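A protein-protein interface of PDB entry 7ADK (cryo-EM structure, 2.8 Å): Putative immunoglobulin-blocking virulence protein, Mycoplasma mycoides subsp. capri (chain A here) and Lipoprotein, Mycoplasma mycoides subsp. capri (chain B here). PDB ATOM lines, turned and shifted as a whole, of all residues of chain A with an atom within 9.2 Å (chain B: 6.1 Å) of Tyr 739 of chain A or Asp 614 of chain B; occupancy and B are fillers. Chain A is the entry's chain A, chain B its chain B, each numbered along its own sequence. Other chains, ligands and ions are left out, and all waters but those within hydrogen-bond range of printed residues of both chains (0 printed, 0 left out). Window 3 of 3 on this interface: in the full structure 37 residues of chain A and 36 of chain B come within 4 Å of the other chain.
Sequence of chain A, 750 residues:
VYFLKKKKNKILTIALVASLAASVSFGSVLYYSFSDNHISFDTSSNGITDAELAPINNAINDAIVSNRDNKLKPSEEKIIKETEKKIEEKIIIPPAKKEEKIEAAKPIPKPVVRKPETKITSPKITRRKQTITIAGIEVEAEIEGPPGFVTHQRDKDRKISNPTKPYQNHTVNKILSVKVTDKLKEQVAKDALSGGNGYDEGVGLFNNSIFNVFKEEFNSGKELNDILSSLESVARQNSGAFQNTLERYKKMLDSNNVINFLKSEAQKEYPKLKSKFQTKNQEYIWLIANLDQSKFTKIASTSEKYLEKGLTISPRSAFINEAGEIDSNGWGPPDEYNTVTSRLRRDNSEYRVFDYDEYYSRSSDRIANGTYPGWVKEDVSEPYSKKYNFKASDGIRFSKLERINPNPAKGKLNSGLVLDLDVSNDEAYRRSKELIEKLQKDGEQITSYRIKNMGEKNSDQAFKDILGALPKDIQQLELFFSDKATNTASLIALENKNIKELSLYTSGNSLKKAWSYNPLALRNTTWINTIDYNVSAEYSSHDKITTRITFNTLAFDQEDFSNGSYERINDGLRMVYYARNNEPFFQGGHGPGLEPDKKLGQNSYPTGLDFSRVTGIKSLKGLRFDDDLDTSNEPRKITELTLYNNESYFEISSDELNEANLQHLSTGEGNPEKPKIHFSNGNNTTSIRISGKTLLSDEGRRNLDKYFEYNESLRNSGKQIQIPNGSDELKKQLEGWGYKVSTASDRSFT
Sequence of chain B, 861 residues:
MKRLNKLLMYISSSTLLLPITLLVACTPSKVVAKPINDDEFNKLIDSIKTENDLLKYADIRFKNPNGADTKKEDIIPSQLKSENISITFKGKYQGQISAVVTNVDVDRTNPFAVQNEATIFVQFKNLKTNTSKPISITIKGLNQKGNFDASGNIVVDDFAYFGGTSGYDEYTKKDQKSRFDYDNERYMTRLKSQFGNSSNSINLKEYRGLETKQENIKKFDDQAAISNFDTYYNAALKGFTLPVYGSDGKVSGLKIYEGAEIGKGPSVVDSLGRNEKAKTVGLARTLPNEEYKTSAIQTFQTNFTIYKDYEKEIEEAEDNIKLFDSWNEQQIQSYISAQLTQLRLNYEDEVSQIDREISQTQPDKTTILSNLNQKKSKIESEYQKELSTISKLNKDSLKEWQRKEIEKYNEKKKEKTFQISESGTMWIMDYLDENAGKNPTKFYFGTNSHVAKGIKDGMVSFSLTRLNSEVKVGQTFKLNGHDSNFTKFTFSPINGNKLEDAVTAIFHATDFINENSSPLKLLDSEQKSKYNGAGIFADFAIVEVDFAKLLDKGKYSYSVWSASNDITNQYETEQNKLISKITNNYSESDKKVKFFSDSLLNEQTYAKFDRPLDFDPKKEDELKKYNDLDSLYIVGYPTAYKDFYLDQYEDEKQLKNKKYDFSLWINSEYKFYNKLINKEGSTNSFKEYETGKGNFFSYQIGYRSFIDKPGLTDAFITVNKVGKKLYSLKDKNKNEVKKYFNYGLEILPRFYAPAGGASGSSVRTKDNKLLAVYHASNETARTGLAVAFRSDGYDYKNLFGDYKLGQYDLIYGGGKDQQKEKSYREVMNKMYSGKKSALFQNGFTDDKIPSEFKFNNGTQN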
ATOM      1  N   SER A 648      -2.399  -9.027   2.209  1.00  0.00           N
ATOM      2  CA  SER A 648      -1.367  -9.755   2.969  1.00  0.00           C
ATOM      3  C   SER A 648      -0.457 -10.639   2.109  1.00  0.00           C
ATOM      4  O   SER A 648       0.623 -11.016   2.542  1.00  0.00           O
ATOM      5  CB  SER A 648      -2.033 -10.619   4.033  1.00  0.00           C
ATOM      6  OG  SER A 648      -2.839 -11.613   3.429  1.00  0.00           O
ATOM      7  N   TYR A 649      -0.887 -10.967   0.895  1.00  0.00           N
ATOM      8  CA  TYR A 649      -0.134 -11.700  -0.105  1.00  0.00           C
ATOM      9  C   TYR A 649       0.401 -10.754  -1.184  1.00  0.00           C
ATOM     10  O   TYR A 649      -0.297  -9.865  -1.660  1.00  0.00           O
ATOM     11  CB  TYR A 649      -1.002 -12.828  -0.685  1.00  0.00           C
ATOM     12  CG  TYR A 649      -2.342 -12.411  -1.263  1.00  0.00           C
ATOM     13  CD1 TYR A 649      -3.488 -12.388  -0.452  1.00  0.00           C
ATOM     14  CD2 TYR A 649      -2.445 -12.060  -2.616  1.00  0.00           C
ATOM     15  CE1 TYR A 649      -4.728 -12.007  -0.994  1.00  0.00           C
ATOM     16  CE2 TYR A 649      -3.687 -11.685  -3.164  1.00  0.00           C
ATOM     17  CZ  TYR A 649      -4.834 -11.654  -2.351  1.00  0.00           C
ATOM     18  OH  TYR A 649      -6.033 -11.300  -2.880  1.00  0.00           O
ATOM     19  N   THR A 686       1.860 -13.013   4.922  1.00  0.00           N
ATOM     20  CA  THR A 686       1.424 -14.130   4.063  1.00  0.00           C
ATOM     21  C   THR A 686       2.302 -14.168   2.796  1.00  0.00           C
ATOM     22  O   THR A 686       3.164 -13.324   2.559  1.00  0.00           O
ATOM     23  CB  THR A 686      -0.101 -14.060   3.815  1.00  0.00           C
ATOM     24  OG1 THR A 686      -0.738 -14.267   5.051  1.00  0.00           O
ATOM     25  CG2 THR A 686      -0.716 -15.112   2.890  1.00  0.00           C
ATOM     26  N   ARG A 689       2.017 -14.937  -3.611  1.00  0.00           N
ATOM     27  CA  ARG A 689       1.043 -15.720  -4.372  1.00  0.00           C
ATOM     28  C   ARG A 689       1.455 -15.718  -5.834  1.00  0.00           C
ATOM     29  O   ARG A 689       1.416 -14.678  -6.484  1.00  0.00           O
ATOM     30  CB  ARG A 689      -0.365 -15.155  -4.138  1.00  0.00           C
ATOM     31  CG  ARG A 689      -1.436 -15.774  -5.058  1.00  0.00           C
ATOM     32  CD  ARG A 689      -2.845 -15.214  -4.850  1.00  0.00           C
ATOM     33  NE  ARG A 689      -3.421 -15.528  -3.528  1.00  0.00           N
ATOM     34  CZ  ARG A 689      -4.668 -15.285  -3.168  1.00  0.00           C
ATOM     35  NH1 ARG A 689      -5.554 -14.808  -3.988  1.00  0.00           N
ATOM     36  NH2 ARG A 689      -5.061 -15.510  -1.958  1.00  0.00           N
ATOM     37  N   ILE A 721       2.766 -19.345  -2.257  1.00  0.00           N
ATOM     38  CA  ILE A 721       1.420 -19.848  -2.561  1.00  0.00           C
ATOM     39  C   ILE A 721       1.366 -20.173  -4.052  1.00  0.00           C
ATOM     40  O   ILE A 721       1.721 -19.331  -4.867  1.00  0.00           O
ATOM     41  CB  ILE A 721       0.332 -18.837  -2.123  1.00  0.00           C
ATOM     42  CG1 ILE A 721      -0.110 -19.102  -0.674  1.00  0.00           C
ATOM     43  CG2 ILE A 721      -0.879 -18.861  -3.061  1.00  0.00           C
ATOM     44  CD1 ILE A 721      -0.901 -17.960  -0.022  1.00  0.00           C
ATOM     45  N   LEU A 734       1.839 -23.321   0.222  1.00  0.00           N
ATOM     46  CA  LEU A 734       0.432 -23.509   0.579  1.00  0.00           C
ATOM     47  C   LEU A 734      -0.479 -23.443  -0.670  1.00  0.00           C
ATOM     48  O   LEU A 734      -0.165 -22.777  -1.654  1.00  0.00           O
ATOM     49  CB  LEU A 734       0.097 -22.426   1.632  1.00  0.00           C
ATOM     50  CG  LEU A 734      -1.365 -22.319   2.101  1.00  0.00           C
ATOM     51  CD1 LEU A 734      -1.807 -23.553   2.886  1.00  0.00           C
ATOM     52  CD2 LEU A 734      -1.569 -21.082   2.971  1.00  0.00           C
ATOM     53  N   GLY A 736      -3.002 -21.728  -1.524  1.00  0.00           N
ATOM     54  CA  GLY A 736      -3.567 -20.423  -1.894  1.00  0.00           C
ATOM     55  C   GLY A 736      -4.931 -20.085  -1.309  1.00  0.00           C
ATOM     56  O   GLY A 736      -5.812 -19.651  -2.042  1.00  0.00           O
ATOM     57  N   TRP A 737      -5.106 -20.275  -0.003  1.00  0.00           N
ATOM     58  CA  TRP A 737      -6.405 -20.202   0.674  1.00  0.00           C
ATOM     59  C   TRP A 737      -7.076 -18.820   0.604  1.00  0.00           C
ATOM     60  O   TRP A 737      -8.233 -18.712   0.197  1.00  0.00           O
ATOM     61  CB  TRP A 737      -6.217 -20.666   2.129  1.00  0.00           C
ATOM     62  CG  TRP A 737      -7.449 -20.889   2.960  1.00  0.00           C
ATOM     63  CD1 TRP A 737      -8.698 -21.114   2.499  1.00  0.00           C
ATOM     64  CD2 TRP A 737      -7.539 -21.021   4.418  1.00  0.00           C
ATOM     65  NE1 TRP A 737      -9.551 -21.345   3.557  1.00  0.00           N
ATOM     66  CE2 TRP A 737      -8.891 -21.312   4.765  1.00  0.00           C
ATOM     67  CE3 TRP A 737      -6.623 -20.918   5.488  1.00  0.00           C
ATOM     68  CZ2 TRP A 737      -9.313 -21.487   6.089  1.00  0.00           C
ATOM     69  CZ3 TRP A 737      -7.037 -21.080   6.825  1.00  0.00           C
ATOM     70  CH2 TRP A 737      -8.380 -21.357   7.127  1.00  0.00           C
ATOM     71  N   GLY A 738      -6.346 -17.758   0.955  1.00  0.00           N
ATOM     72  CA  GLY A 738      -6.860 -16.382   0.973  1.00  0.00           C
ATOM     73  C   GLY A 738      -7.862 -16.138   2.105  1.00  0.00           C
ATOM     74  O   GLY A 738      -9.021 -15.827   1.854  1.00  0.00           O
ATOM     75  N   TYR A 739      -7.430 -16.317   3.353  1.00  0.00           N
ATOM     76  CA  TYR A 739      -8.304 -16.282   4.525  1.00  0.00           C
ATOM     77  C   TYR A 739      -7.509 -15.680   5.693  1.00  0.00           C
ATOM     78  O   TYR A 739      -6.463 -16.218   6.052  1.00  0.00           O
ATOM     79  CB  TYR A 739      -8.724 -17.738   4.802  1.00  0.00           C
ATOM     80  CG  TYR A 739     -10.025 -17.953   5.536  1.00  0.00           C
ATOM     81  CD1 TYR A 739     -11.155 -18.383   4.820  1.00  0.00           C
ATOM     82  CD2 TYR A 739     -10.092 -17.808   6.930  1.00  0.00           C
ATOM     83  CE1 TYR A 739     -12.349 -18.676   5.499  1.00  0.00           C
ATOM     84  CE2 TYR A 739     -11.293 -18.078   7.609  1.00  0.00           C
ATOM     85  CZ  TYR A 739     -12.422 -18.516   6.896  1.00  0.00           C
ATOM     86  OH  TYR A 739     -13.588 -18.757   7.539  1.00  0.00           O
ATOM     87  N   LYS A 740      -7.944 -14.541   6.233  1.00  0.00           N
ATOM     88  CA  LYS A 740      -7.402 -13.906   7.450  1.00  0.00           C
ATOM     89  C   LYS A 740      -8.316 -12.782   7.933  1.00  0.00           C
ATOM     90  O   LYS A 740      -8.866 -12.890   9.025  1.00  0.00           O
ATOM     91  CB  LYS A 740      -5.981 -13.341   7.263  1.00  0.00           C
ATOM     92  CG  LYS A 740      -5.200 -13.302   8.591  1.00  0.00           C
ATOM     93  CD  LYS A 740      -4.614 -14.649   8.990  1.00  0.00           C
ATOM     94  CE  LYS A 740      -3.829 -14.625  10.291  1.00  0.00           C
ATOM     95  NZ  LYS A 740      -3.285 -15.945  10.621  1.00  0.00           N
ATOM     96  N   TYR B 168      -4.431 -25.775  14.090  1.00  0.00           N
ATOM     97  CA  TYR B 168      -5.049 -24.455  14.112  1.00  0.00           C
ATOM     98  C   TYR B 168      -6.515 -24.488  13.645  1.00  0.00           C
ATOM     99  O   TYR B 168      -7.372 -23.938  14.333  1.00  0.00           O
ATOM    100  CB  TYR B 168      -4.193 -23.474  13.308  1.00  0.00           C
ATOM    101  CG  TYR B 168      -4.857 -22.131  13.112  1.00  0.00           C
ATOM    102  CD1 TYR B 168      -4.915 -21.206  14.170  1.00  0.00           C
ATOM    103  CD2 TYR B 168      -5.464 -21.835  11.881  1.00  0.00           C
ATOM    104  CE1 TYR B 168      -5.590 -19.988  13.996  1.00  0.00           C
ATOM    105  CE2 TYR B 168      -6.134 -20.621  11.704  1.00  0.00           C
ATOM    106  CZ  TYR B 168      -6.205 -19.699  12.765  1.00  0.00           C
ATOM    107  OH  TYR B 168      -6.893 -18.548  12.600  1.00  0.00           O
ATOM    108  N   ASP B 169      -6.845 -25.186  12.550  1.00  0.00           N
ATOM    109  CA  ASP B 169      -8.229 -25.308  12.071  1.00  0.00           C
ATOM    110  C   ASP B 169      -9.188 -25.808  13.151  1.00  0.00           C
ATOM    111  O   ASP B 169     -10.279 -25.263  13.296  1.00  0.00           O
ATOM    112  CB  ASP B 169      -8.306 -26.256  10.863  1.00  0.00           C
ATOM    113  CG  ASP B 169      -8.037 -25.616   9.505  1.00  0.00           C
ATOM    114  OD1 ASP B 169      -8.076 -24.378   9.378  1.00  0.00           O
ATOM    115  OD2 ASP B 169      -7.879 -26.367   8.521  1.00  0.00           O
ATOM    116  N   THR B 172      -9.854 -22.957  15.602  1.00  0.00           N
ATOM    117  CA  THR B 172     -10.854 -22.031  15.052  1.00  0.00           C
ATOM    118  C   THR B 172     -12.281 -22.532  15.284  1.00  0.00           C
ATOM    119  O   THR B 172     -13.168 -21.725  15.544  1.00  0.00           O
ATOM    120  CB  THR B 172     -10.666 -21.700  13.558  1.00  0.00           C
ATOM    121  OG1 THR B 172     -11.132 -22.719  12.708  1.00  0.00           O
ATOM    122  CG2 THR B 172      -9.250 -21.381  13.157  1.00  0.00           C
ATOM    123  N   ARG B 611     -14.652 -11.539  18.770  1.00  0.00           N
ATOM    124  CA  ARG B 611     -14.092 -11.578  17.411  1.00  0.00           C
ATOM    125  C   ARG B 611     -13.898 -13.003  16.861  1.00  0.00           C
ATOM    126  O   ARG B 611     -13.505 -13.888  17.622  1.00  0.00           O
ATOM    127  CB  ARG B 611     -12.770 -10.790  17.366  1.00  0.00           C
ATOM    128  CG  ARG B 611     -11.576 -11.496  18.025  1.00  0.00           C
ATOM    129  CD  ARG B 611     -10.333 -10.624  18.028  1.00  0.00           C
ATOM    130  NE  ARG B 611      -9.156 -11.310  18.583  1.00  0.00           N
ATOM    131  CZ  ARG B 611      -8.211 -11.928  17.906  1.00  0.00           C
ATOM    132  NH1 ARG B 611      -7.199 -12.438  18.526  1.00  0.00           N
ATOM    133  NH2 ARG B 611      -8.248 -12.048  16.621  1.00  0.00           N
ATOM    134  N   PRO B 612     -14.041 -13.244  15.545  1.00  0.00           N
ATOM    135  CA  PRO B 612     -13.479 -14.433  14.917  1.00  0.00           C
ATOM    136  C   PRO B 612     -11.946 -14.329  14.880  1.00  0.00           C
ATOM    137  O   PRO B 612     -11.403 -13.237  14.737  1.00  0.00           O
ATOM    138  CB  PRO B 612     -14.089 -14.445  13.523  1.00  0.00           C
ATOM    139  CG  PRO B 612     -14.268 -12.979  13.184  1.00  0.00           C
ATOM    140  CD  PRO B 612     -14.557 -12.340  14.535  1.00  0.00           C
ATOM    141  N   LEU B 613     -11.214 -15.444  14.986  1.00  0.00           N
ATOM    142  CA  LEU B 613      -9.742 -15.420  14.895  1.00  0.00           C
ATOM    143  C   LEU B 613      -9.274 -15.042  13.485  1.00  0.00           C
ATOM    144  O   LEU B 613      -8.276 -14.346  13.317  1.00  0.00           O
ATOM    145  CB  LEU B 613      -9.138 -16.783  15.250  1.00  0.00           C
ATOM    146  CG  LEU B 613      -9.544 -17.366  16.603  1.00  0.00           C
ATOM    147  CD1 LEU B 613      -8.970 -18.768  16.737  1.00  0.00           C
ATOM    148  CD2 LEU B 613      -9.081 -16.517  17.784  1.00  0.00           C
ATOM    149  N   ASP B 614     -10.018 -15.500  12.480  1.00  0.00           N
ATOM    150  CA  ASP B 614      -9.853 -15.242  11.061  1.00  0.00           C
ATOM    151  C   ASP B 614     -11.206 -15.254  10.346  1.00  0.00           C
ATOM    152  O   ASP B 614     -12.193 -15.814  10.827  1.00  0.00           O
ATOM    153  CB  ASP B 614      -8.906 -16.263  10.428  1.00  0.00           C
ATOM    154  CG  ASP B 614      -9.253 -17.733  10.677  1.00  0.00           C
ATOM    155  OD1 ASP B 614     -10.348 -18.085  11.163  1.00  0.00           O
ATOM    156  OD2 ASP B 614      -8.372 -18.563  10.387  1.00  0.00           O
ATOM    157  N   PHE B 615     -11.271 -14.645   9.173  1.00  0.00           N
ATOM    158  CA  PHE B 615     -12.461 -14.585   8.334  1.00  0.00           C
ATOM    159  C   PHE B 615     -12.036 -14.501   6.872  1.00  0.00           C
ATOM    160  O   PHE B 615     -10.881 -14.201   6.584  1.00  0.00           O
ATOM    161  CB  PHE B 615     -13.360 -13.412   8.759  1.00  0.00           C
ATOM    162  CG  PHE B 615     -12.950 -12.032   8.287  1.00  0.00           C
ATOM    163  CD1 PHE B 615     -11.738 -11.460   8.697  1.00  0.00           C
ATOM    164  CD2 PHE B 615     -13.814 -11.291   7.470  1.00  0.00           C
ATOM    165  CE1 PHE B 615     -11.375 -10.178   8.268  1.00  0.00           C
ATOM    166  CE2 PHE B 615     -13.466  -9.998   7.062  1.00  0.00           C
ATOM    167  CZ  PHE B 615     -12.241  -9.450   7.445  1.00  0.00           C
ATOM    168  N   ASP B 616     -12.942 -14.773   5.939  1.00  0.00           N
ATOM    169  CA  ASP B 616     -12.715 -14.536   4.520  1.00  0.00           C
ATOM    170  C   ASP B 616     -13.083 -13.083   4.158  1.00  0.00           C
ATOM    171  O   ASP B 616     -14.267 -12.743   4.118  1.00  0.00           O
ATOM    172  CB  ASP B 616     -13.515 -15.557   3.717  1.00  0.00           C
ATOM    173  CG  ASP B 616     -13.202 -15.528   2.225  1.00  0.00           C
ATOM    174  OD1 ASP B 616     -12.535 -14.587   1.741  1.00  0.00           O
ATOM    175  OD2 ASP B 616     -13.658 -16.449   1.513  1.00  0.00           O
ATOM    176  N   PRO B 617     -12.128 -12.177   3.871  1.00  0.00           N
ATOM    177  CA  PRO B 617     -12.453 -10.789   3.540  1.00  0.00           C
ATOM    178  C   PRO B 617     -13.143 -10.650   2.182  1.00  0.00           C
ATOM    179  O   PRO B 617     -13.753  -9.625   1.901  1.00  0.00           O
ATOM    180  CB  PRO B 617     -11.120 -10.054   3.569  1.00  0.00           C
ATOM    181  CG  PRO B 617     -10.108 -11.129   3.214  1.00  0.00           C
ATOM    182  CD  PRO B 617     -10.691 -12.383   3.834  1.00  0.00           C
ATOM    183  N   LYS B 618     -13.046 -11.673   1.325  1.00  0.00           N
ATOM    184  CA  LYS B 618     -13.586 -11.680  -0.045  1.00  0.00           C
ATOM    185  C   LYS B 618     -15.060 -12.097  -0.092  1.00  0.00           C
ATOM    186  O   LYS B 618     -15.774 -11.759  -1.034  1.00  0.00           O
ATOM    187  CB  LYS B 618     -12.760 -12.643  -0.915  1.00  0.00           C
ATOM    188  CG  LYS B 618     -11.236 -12.565  -0.703  1.00  0.00           C
ATOM    189  CD  LYS B 618     -10.411 -13.517  -1.585  1.00  0.00           C
ATOM    190  CE  LYS B 618     -10.839 -14.993  -1.590  1.00  0.00           C
ATOM    191  NZ  LYS B 618     -10.921 -15.607  -0.245  1.00  0.00           N
ATOM    192  N   ASP B 621     -19.737 -12.243   4.308  1.00  0.00           N
ATOM    193  CA  ASP B 621     -19.724 -12.075   5.776  1.00  0.00           C
ATOM    194  C   ASP B 621     -18.603 -11.142   6.308  1.00  0.00           C
ATOM    195  O   ASP B 621     -18.014 -11.366   7.364  1.00  0.00           O
ATOM    196  CB  ASP B 621     -19.823 -13.424   6.511  1.00  0.00           C
ATOM    197  CG  ASP B 621     -18.572 -14.301   6.498  1.00  0.00           C
ATOM    198  OD1 ASP B 621     -17.621 -14.021   5.744  1.00  0.00           O
ATOM    199  OD2 ASP B 621     -18.552 -15.302   7.246  1.00  0.00           O
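Among the printed residues, 8 pairs touch across the chains. Among the printed residues, no Asp or Glu carboxylate lies within 4 Å of a Lys or Arg side-chain nitrogen of the other chain.
The side-chain hydroxyl (OH) of Tyr 168 of chain B is in hydrogen-bond range of the side-chain carboxylate (OD2) of Asp 614 of chain B (2.7 Å). The side-chain carboxylate of Asp 616 of chain B is in salt-bridge range of the side-chain amino group of Lys 618 of chain B, 2.8 Å away. O of Asp 169 of chain B is in hydrogen-bond range of OG1 of Thr 172 of chain B (2.7 Å).
O of Gly 738 of chain A is in hydrogen-bond range of NZ of Lys 618 of chain B. The backbone NH of Lys 740 of chain A lies within hydrogen-bond range of the backbone carbonyl oxygen of Phe 615 of chain B.
Asp 169 of chain B touches Trp 737 of chain A (OD1 to CH2, 3.8 Å). Asp 616 of chain B touches Gly 738 of chain A (OD1 to O, 3.7 Å). Asp 614 of chain B touches Tyr 739 of chain A (OD1 to CE2, 3.7 Å). Tyr 739 of chain A touches Phe 615 of chain B. Asp 616 of chain B touches Tyr 739 of chain A. CA of Asp 614 of chain B touches O of Lys 740 of chain A, at 3.3 Å.
Of chain B, only Asp 614 (3.7 Å), Phe 615 (3.7 Å) and Asp 616 (3.8 Å) come within 4 Å of Tyr 739 of chain A. Of the printed residues of chain B, Lys 740 of chain A touches Asp 614 and Phe 615. Asp 614 of chain B touches just these residues of chain A: Tyr 739 and Lys 740. Of the printed residues of chain A, Asp 616 of chain B touches Gly 738 and Tyr 739. Printed residues of chain A within 4 Å of Lys 618 of chain B: Gly 738 (2.8 Å). The nearest residue of chain B that does not touch Tyr 739 of chain A is Pro 617 of chain B (4.6 Å). The nearest residue of chain A that does not touch Asp 614 of chain B is Trp 737 of chain A (4.3 Å). The nearest printed residue of chain B that does not touch Trp 737 of chain A is Lys 618 of chain B (4.1 Å).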
